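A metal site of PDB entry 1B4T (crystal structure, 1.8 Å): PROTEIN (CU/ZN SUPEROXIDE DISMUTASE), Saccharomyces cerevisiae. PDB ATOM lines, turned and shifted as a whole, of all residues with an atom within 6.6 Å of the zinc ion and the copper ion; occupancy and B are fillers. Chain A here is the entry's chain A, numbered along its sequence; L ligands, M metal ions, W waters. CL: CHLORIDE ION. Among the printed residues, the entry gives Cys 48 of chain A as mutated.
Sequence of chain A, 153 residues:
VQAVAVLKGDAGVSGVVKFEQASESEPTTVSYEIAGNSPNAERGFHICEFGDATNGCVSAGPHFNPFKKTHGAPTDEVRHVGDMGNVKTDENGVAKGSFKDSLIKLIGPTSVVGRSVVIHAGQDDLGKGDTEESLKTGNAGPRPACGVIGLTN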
ATOM      1  N   GLY A  44       4.575  14.359  -2.201  1.00  0.00           N
ATOM      2  CA  GLY A  44       5.072  13.411  -3.183  1.00  0.00           C
ATOM      3  C   GLY A  44       6.502  13.733  -3.557  1.00  0.00           C
ATOM      4  O   GLY A  44       6.803  14.875  -3.851  1.00  0.00           O
ATOM      5  N   PHE A  45       7.345  12.707  -3.628  1.00  0.00           N
ATOM      6  CA  PHE A  45       8.780  12.830  -3.921  1.00  0.00           C
ATOM      7  C   PHE A  45       9.059  11.795  -5.005  1.00  0.00           C
ATOM      8  O   PHE A  45       9.054  10.602  -4.709  1.00  0.00           O
ATOM      9  CB  PHE A  45       9.521  12.491  -2.634  1.00  0.00           C
ATOM     10  CG  PHE A  45      10.992  12.739  -2.664  1.00  0.00           C
ATOM     11  CD1 PHE A  45      11.511  13.918  -3.169  1.00  0.00           C
ATOM     12  CD2 PHE A  45      11.870  11.815  -2.111  1.00  0.00           C
ATOM     13  CE1 PHE A  45      12.894  14.182  -3.116  1.00  0.00           C
ATOM     14  CE2 PHE A  45      13.242  12.065  -2.043  1.00  0.00           C
ATOM     15  CZ  PHE A  45      13.753  13.240  -2.544  1.00  0.00           C
ATOM     16  N   HIS A  46       9.297  12.242  -6.241  1.00  0.00           N
ATOM     17  CA  HIS A  46       9.503  11.300  -7.353  1.00  0.00           C
ATOM     18  C   HIS A  46      10.649  11.618  -8.286  1.00  0.00           C
ATOM     19  O   HIS A  46      11.137  12.731  -8.339  1.00  0.00           O
ATOM     20  CB  HIS A  46       8.250  11.235  -8.232  1.00  0.00           C
ATOM     21  CG  HIS A  46       6.972  11.084  -7.467  1.00  0.00           C
ATOM     22  ND1 HIS A  46       5.867  11.882  -7.699  1.00  0.00           N
ATOM     23  CD2 HIS A  46       6.610  10.236  -6.478  1.00  0.00           C
ATOM     24  CE1 HIS A  46       4.884  11.530  -6.888  1.00  0.00           C
ATOM     25  NE2 HIS A  46       5.312  10.533  -6.133  1.00  0.00           N
ATOM     26  N   ILE A  47      11.088  10.588  -9.004  1.00  0.00           N
ATOM     27  CA  ILE A  47      12.126  10.744 -10.015  1.00  0.00           C
ATOM     28  C   ILE A  47      11.432  10.618 -11.374  1.00  0.00           C
ATOM     29  O   ILE A  47      10.710   9.642 -11.619  1.00  0.00           O
ATOM     30  CB  ILE A  47      13.222   9.684  -9.913  1.00  0.00           C
ATOM     31  CG1 ILE A  47      13.984   9.845  -8.604  1.00  0.00           C
ATOM     32  CG2 ILE A  47      14.187   9.803 -11.105  1.00  0.00           C
ATOM     33  CD1 ILE A  47      14.980   8.737  -8.335  1.00  0.00           C
ATOM     34  N   CYS A  48      11.619  11.603 -12.235  1.00  0.00           N
ATOM     35  CA  CYS A  48      11.015  11.619 -13.569  1.00  0.00           C
ATOM     36  C   CYS A  48      11.982  11.185 -14.667  1.00  0.00           C
ATOM     37  O   CYS A  48      13.204  11.219 -14.503  1.00  0.00           O
ATOM     38  CB  CYS A  48      10.370  12.986 -13.859  1.00  0.00           C
ATOM     39  SG  CYS A  48       8.930  13.329 -12.835  1.00  0.00           S
ATOM     40  N   HIS A  63       6.899   9.869 -14.403  1.00  0.00           N
ATOM     41  CA  HIS A  63       7.773   9.155 -13.487  1.00  0.00           C
ATOM     42  C   HIS A  63       8.604   8.147 -14.281  1.00  0.00           C
ATOM     43  O   HIS A  63       8.105   7.563 -15.249  1.00  0.00           O
ATOM     44  CB  HIS A  63       6.939   8.414 -12.476  1.00  0.00           C
ATOM     45  CG  HIS A  63       6.154   9.304 -11.585  1.00  0.00           C
ATOM     46  ND1 HIS A  63       5.133   8.842 -10.788  1.00  0.00           N
ATOM     47  CD2 HIS A  63       6.276  10.632 -11.304  1.00  0.00           C
ATOM     48  CE1 HIS A  63       4.659   9.832 -10.056  1.00  0.00           C
ATOM     49  NE2 HIS A  63       5.342  10.925 -10.349  1.00  0.00           N
ATOM     50  N   PHE A  64       9.865   7.949 -13.883  1.00  0.00           N
ATOM     51  CA  PHE A  64      10.730   6.996 -14.559  1.00  0.00           C
ATOM     52  C   PHE A  64      10.068   5.616 -14.383  1.00  0.00           C
ATOM     53  O   PHE A  64       9.832   5.169 -13.265  1.00  0.00           O
ATOM     54  CB  PHE A  64      12.129   7.047 -13.984  1.00  0.00           C
ATOM     55  CG  PHE A  64      13.134   6.268 -14.770  1.00  0.00           C
ATOM     56  CD1 PHE A  64      13.085   6.241 -16.163  1.00  0.00           C
ATOM     57  CD2 PHE A  64      14.142   5.554 -14.117  1.00  0.00           C
ATOM     58  CE1 PHE A  64      14.017   5.525 -16.887  1.00  0.00           C
ATOM     59  CE2 PHE A  64      15.088   4.830 -14.845  1.00  0.00           C
ATOM     60  CZ  PHE A  64      15.019   4.817 -16.240  1.00  0.00           C
ATOM     61  N   THR A  70       2.356   0.392 -13.020  1.00  0.00           N
ATOM     62  CA  THR A  70       1.555   1.519 -12.530  1.00  0.00           C
ATOM     63  C   THR A  70       2.182   2.153 -11.290  1.00  0.00           C
ATOM     64  O   THR A  70       3.117   1.606 -10.714  1.00  0.00           O
ATOM     65  CB  THR A  70       0.087   1.114 -12.214  1.00  0.00           C
ATOM     66  OG1 THR A  70       0.081  -0.065 -11.405  1.00  0.00           O
ATOM     67  CG2 THR A  70      -0.688   0.860 -13.496  1.00  0.00           C
ATOM     68  N   HIS A  71       1.664   3.317 -10.907  1.00  0.00           N
ATOM     69  CA  HIS A  71       2.162   4.045  -9.756  1.00  0.00           C
ATOM     70  C   HIS A  71       1.808   3.344  -8.441  1.00  0.00           C
ATOM     71  O   HIS A  71       0.655   2.950  -8.219  1.00  0.00           O
ATOM     72  CB  HIS A  71       1.600   5.478  -9.749  1.00  0.00           C
ATOM     73  CG  HIS A  71       2.129   6.325  -8.638  1.00  0.00           C
ATOM     74  ND1 HIS A  71       3.318   7.024  -8.732  1.00  0.00           N
ATOM     75  CD2 HIS A  71       1.688   6.515  -7.371  1.00  0.00           C
ATOM     76  CE1 HIS A  71       3.591   7.592  -7.576  1.00  0.00           C
ATOM     77  NE2 HIS A  71       2.618   7.297  -6.738  1.00  0.00           N
ATOM     78  N   GLY A  72       2.792   3.237  -7.559  1.00  0.00           N
ATOM     79  CA  GLY A  72       2.578   2.587  -6.281  1.00  0.00           C
ATOM     80  C   GLY A  72       3.455   3.200  -5.220  1.00  0.00           C
ATOM     81  O   GLY A  72       4.029   4.268  -5.414  1.00  0.00           O
ATOM     82  N   ARG A  79       5.201  -0.785  -8.990  1.00  0.00           N
ATOM     83  CA  ARG A  79       5.444   0.635  -8.792  1.00  0.00           C
ATOM     84  C   ARG A  79       6.389   1.082  -9.896  1.00  0.00           C
ATOM     85  O   ARG A  79       7.025   0.272 -10.569  1.00  0.00           O
ATOM     86  CB  ARG A  79       6.124   0.880  -7.443  1.00  0.00           C
ATOM     87  CG  ARG A  79       7.423   0.096  -7.251  1.00  0.00           C
ATOM     88  CD  ARG A  79       8.267   0.586  -6.087  1.00  0.00           C
ATOM     89  NE  ARG A  79       9.319   1.514  -6.489  1.00  0.00           N
ATOM     90  CZ  ARG A  79      10.471   1.688  -5.845  1.00  0.00           C
ATOM     91  NH1 ARG A  79      10.742   0.986  -4.751  1.00  0.00           N
ATOM     92  NH2 ARG A  79      11.387   2.534  -6.307  1.00  0.00           N
ATOM     93  N   HIS A  80       6.484   2.387 -10.075  1.00  0.00           N
ATOM     94  CA  HIS A  80       7.410   2.965 -11.041  1.00  0.00           C
ATOM     95  C   HIS A  80       8.765   2.971 -10.332  1.00  0.00           C
ATOM     96  O   HIS A  80       8.821   2.974  -9.117  1.00  0.00           O
ATOM     97  CB  HIS A  80       7.026   4.407 -11.349  1.00  0.00           C
ATOM     98  CG  HIS A  80       5.694   4.557 -12.005  1.00  0.00           C
ATOM     99  ND1 HIS A  80       4.885   5.659 -11.796  1.00  0.00           N
ATOM    100  CD2 HIS A  80       5.054   3.794 -12.916  1.00  0.00           C
ATOM    101  CE1 HIS A  80       3.815   5.562 -12.564  1.00  0.00           C
ATOM    102  NE2 HIS A  80       3.897   4.442 -13.252  1.00  0.00           N
ATOM    103  N   VAL A  81       9.852   3.017 -11.091  1.00  0.00           N
ATOM    104  CA  VAL A  81      11.189   3.059 -10.479  1.00  0.00           C
ATOM    105  C   VAL A  81      11.357   4.369  -9.695  1.00  0.00           C
ATOM    106  O   VAL A  81      11.902   4.380  -8.596  1.00  0.00           O
ATOM    107  CB  VAL A  81      12.317   2.902 -11.548  1.00  0.00           C
ATOM    108  CG1 VAL A  81      13.660   3.310 -10.976  1.00  0.00           C
ATOM    109  CG2 VAL A  81      12.364   1.465 -12.060  1.00  0.00           C
ATOM    110  N   GLY A  82      10.849   5.464 -10.248  1.00  0.00           N
ATOM    111  CA  GLY A  82      10.947   6.756  -9.593  1.00  0.00           C
ATOM    112  C   GLY A  82       9.958   7.014  -8.468  1.00  0.00           C
ATOM    113  O   GLY A  82       9.802   8.155  -8.023  1.00  0.00           O
ATOM    114  N   ASP A  83       9.279   5.973  -7.997  1.00  0.00           N
ATOM    115  CA  ASP A  83       8.306   6.110  -6.932  1.00  0.00           C
ATOM    116  C   ASP A  83       8.964   6.008  -5.579  1.00  0.00           C
ATOM    117  O   ASP A  83       9.213   4.920  -5.068  1.00  0.00           O
ATOM    118  CB  ASP A  83       7.209   5.060  -7.047  1.00  0.00           C
ATOM    119  CG  ASP A  83       6.234   5.382  -8.159  1.00  0.00           C
ATOM    120  OD1 ASP A  83       6.263   6.514  -8.682  1.00  0.00           O
ATOM    121  OD2 ASP A  83       5.428   4.498  -8.504  1.00  0.00           O
ATOM    122  N   VAL A 118      11.754  15.318  -8.533  1.00  0.00           N
ATOM    123  CA  VAL A 118      10.665  16.272  -8.389  1.00  0.00           C
ATOM    124  C   VAL A 118      10.013  16.162  -7.010  1.00  0.00           C
ATOM    125  O   VAL A 118       9.828  15.050  -6.483  1.00  0.00           O
ATOM    126  CB  VAL A 118       9.592  16.040  -9.511  1.00  0.00           C
ATOM    127  CG1 VAL A 118       8.281  16.738  -9.187  1.00  0.00           C
ATOM    128  CG2 VAL A 118      10.107  16.537 -10.854  1.00  0.00           C
ATOM    129  N   HIS A 120       6.562  17.356  -4.960  1.00  0.00           N
ATOM    130  CA  HIS A 120       5.196  17.779  -5.250  1.00  0.00           C
ATOM    131  C   HIS A 120       4.567  18.746  -4.291  1.00  0.00           C
ATOM    132  O   HIS A 120       5.026  18.863  -3.162  1.00  0.00           O
ATOM    133  CB  HIS A 120       4.283  16.574  -5.371  1.00  0.00           C
ATOM    134  CG  HIS A 120       4.456  15.846  -6.654  1.00  0.00           C
ATOM    135  ND1 HIS A 120       3.882  16.279  -7.833  1.00  0.00           N
ATOM    136  CD2 HIS A 120       5.204  14.770  -6.980  1.00  0.00           C
ATOM    137  CE1 HIS A 120       4.276  15.510  -8.818  1.00  0.00           C
ATOM    138  NE2 HIS A 120       5.083  14.589  -8.328  1.00  0.00           N
ATOM    139  N   ASP A 124       1.021  12.192  -2.297  1.00  0.00           N
ATOM    140  CA  ASP A 124       0.937  11.055  -3.206  1.00  0.00           C
ATOM    141  C   ASP A 124      -0.029  10.026  -2.564  1.00  0.00           C
ATOM    142  O   ASP A 124       0.207   9.557  -1.456  1.00  0.00           O
ATOM    143  CB  ASP A 124       2.371  10.495  -3.324  1.00  0.00           C
ATOM    144  CG  ASP A 124       2.509   9.332  -4.304  1.00  0.00           C
ATOM    145  OD1 ASP A 124       1.515   8.793  -4.802  1.00  0.00           O
ATOM    146  OD2 ASP A 124       3.664   8.948  -4.557  1.00  0.00           O
ATOM    147  N   LEU A 135      -3.099   6.028 -10.713  1.00  0.00           N
ATOM    148  CA  LEU A 135      -2.196   4.998 -11.247  1.00  0.00           C
ATOM    149  C   LEU A 135      -1.045   5.522 -12.064  1.00  0.00           C
ATOM    150  O   LEU A 135      -0.245   4.741 -12.603  1.00  0.00           O
ATOM    151  CB  LEU A 135      -2.974   3.971 -12.083  1.00  0.00           C
ATOM    152  CG  LEU A 135      -3.942   3.053 -11.339  1.00  0.00           C
ATOM    153  CD1 LEU A 135      -4.654   2.203 -12.378  1.00  0.00           C
ATOM    154  CD2 LEU A 135      -3.215   2.199 -10.292  1.00  0.00           C
ATOM    155  N   LYS A 136      -0.967   6.834 -12.221  1.00  0.00           N
ATOM    156  CA  LYS A 136       0.129   7.413 -12.951  1.00  0.00           C
ATOM    157  C   LYS A 136       0.947   8.389 -12.133  1.00  0.00           C
ATOM    158  O   LYS A 136       2.168   8.299 -12.114  1.00  0.00           O
ATOM    159  CB  LYS A 136      -0.350   8.047 -14.255  1.00  0.00           C
ATOM    160  CG  LYS A 136      -1.668   8.744 -14.208  1.00  0.00           C
ATOM    161  CD  LYS A 136      -1.765   9.696 -15.391  1.00  0.00           C
ATOM    162  CE  LYS A 136      -1.376   9.048 -16.726  1.00  0.00           C
ATOM    163  NZ  LYS A 136      -2.254   7.874 -17.084  1.00  0.00           N
ATOM    164  N   THR A 137       0.274   9.271 -11.391  1.00  0.00           N
ATOM    165  CA  THR A 137       0.963  10.282 -10.599  1.00  0.00           C
ATOM    166  C   THR A 137       0.704  10.182  -9.091  1.00  0.00           C
ATOM    167  O   THR A 137       1.400  10.805  -8.278  1.00  0.00           O
ATOM    168  CB  THR A 137       0.578  11.725 -11.054  1.00  0.00           C
ATOM    169  OG1 THR A 137      -0.811  11.975 -10.764  1.00  0.00           O
ATOM    170  CG2 THR A 137       0.785  11.908 -12.535  1.00  0.00           C
ATOM    171  N   GLY A 138      -0.258   9.352  -8.704  1.00  0.00           N
ATOM    172  CA  GLY A 138      -0.572   9.273  -7.307  1.00  0.00           C
ATOM    173  C   GLY A 138      -1.361  10.514  -6.924  1.00  0.00           C
ATOM    174  O   GLY A 138      -1.608  10.745  -5.740  1.00  0.00           O
ATOM    175  N   ALA A 140      -0.538  13.598  -6.928  1.00  0.00           N
ATOM    176  CA  ALA A 140       0.256  14.452  -6.082  1.00  0.00           C
ATOM    177  C   ALA A 140       0.276  15.951  -6.412  1.00  0.00           C
ATOM    178  O   ALA A 140       0.965  16.721  -5.758  1.00  0.00           O
ATOM    179  CB  ALA A 140       1.669  13.877  -5.994  1.00  0.00           C
ATOM    180  N   GLY A 141      -0.433  16.344  -7.464  1.00  0.00           N
ATOM    181  CA  GLY A 141      -0.508  17.760  -7.794  1.00  0.00           C
ATOM    182  C   GLY A 141       0.681  18.373  -8.500  1.00  0.00           C
ATOM    183  O   GLY A 141       1.506  17.653  -9.075  1.00  0.00           O
ATOM    184  N   ARG A 143       4.316  20.533  -9.405  1.00  0.00           N
ATOM    185  CA  ARG A 143       5.707  20.279  -9.119  1.00  0.00           C
ATOM    186  C   ARG A 143       6.385  21.612  -8.804  1.00  0.00           C
ATOM    187  O   ARG A 143       6.895  22.267  -9.714  1.00  0.00           O
ATOM    188  CB  ARG A 143       6.397  19.694 -10.354  1.00  0.00           C
ATOM    189  CG  ARG A 143       5.719  18.496 -10.946  1.00  0.00           C
ATOM    190  CD  ARG A 143       6.343  18.128 -12.268  1.00  0.00           C
ATOM    191  NE  ARG A 143       5.617  17.035 -12.900  1.00  0.00           N
ATOM    192  CZ  ARG A 143       6.080  16.290 -13.896  1.00  0.00           C
ATOM    193  NH1 ARG A 143       7.281  16.521 -14.397  1.00  0.00           N
ATOM    194  NH2 ARG A 143       5.350  15.301 -14.361  1.00  0.00           N
HETATM  195 CL    CL L   1       5.588  13.777 -11.273  1.00  0.00          CL
HETATM  196 ZN    ZN M   1       4.910   6.971 -10.137  1.00  0.00          ZN
HETATM  197 CU    CU M   2       5.368  12.783  -9.406  1.00  0.00          CU
HETATM  198  O   HOH W   1       2.696  12.669  -9.574  1.00  0.00           O
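The backbone carbonyl oxygen (O) of Asp 83 lies within hydrogen-bond range of the guanidinium group (NH2) of Arg 79, 3.5 Å away.
The side-chain carboxylate (OD1) of Asp 124 is in hydrogen-bond range of a ring nitrogen (NE2) of His 71, at 2.7 Å.
The side-chain carboxylate of Asp 83 sits at hydrogen-bond distance from the backbone NH of Gly 72, at 3.1 Å.
A ring nitrogen (ND1) of His 63 sits close to the backbone carbonyl oxygen of Lys 136 (3.3 Å).
The backbone carbonyl oxygen (O) of Gly 141 sits at hydrogen-bond distance from a ring nitrogen (ND1) of His 120, 3.0 Å away.
The backbone NH (N) of Val 118 is in hydrogen-bond range of the backbone carbonyl oxygen (O) of His 46, 2.7 Å away.
NE2 of His 46 lies within hydrogen-bond range of OD2 of Asp 124 (2.8 Å).
O of Gly 44 lies within hydrogen-bond range of N of His 120 (2.7 Å).
Residues that only touch the zinc ion: Lys 136.
Within 4 Å of the zinc ion: His 63, His 71, His 80, Asp 83 and Lys 136.
Within 4 Å of the copper ion: His 46, His 63 and His 120.
ND1 of His 63 is bound to the zinc ion (2.0 Å).
OD1 of Asp 83 binds the zinc ion (2.0 Å).
A ring nitrogen (ND1) of His 80 is bound to the zinc ion (2.1 Å).
A ring nitrogen (ND1) of His 71 binds the zinc ion (2.1 Å).
ND1 of His 46 binds the copper ion.
A ring nitrogen (NE2) of His 63 binds the copper ion (2.1 Å).
The copper ion is bound by NE2 of His 120, 2.1 Å away.
A chlorine (CL) of the ligand is bound to the copper ion (2.1 Å).
Slightly farther from the copper ion lies water W1 (2.7 Å).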
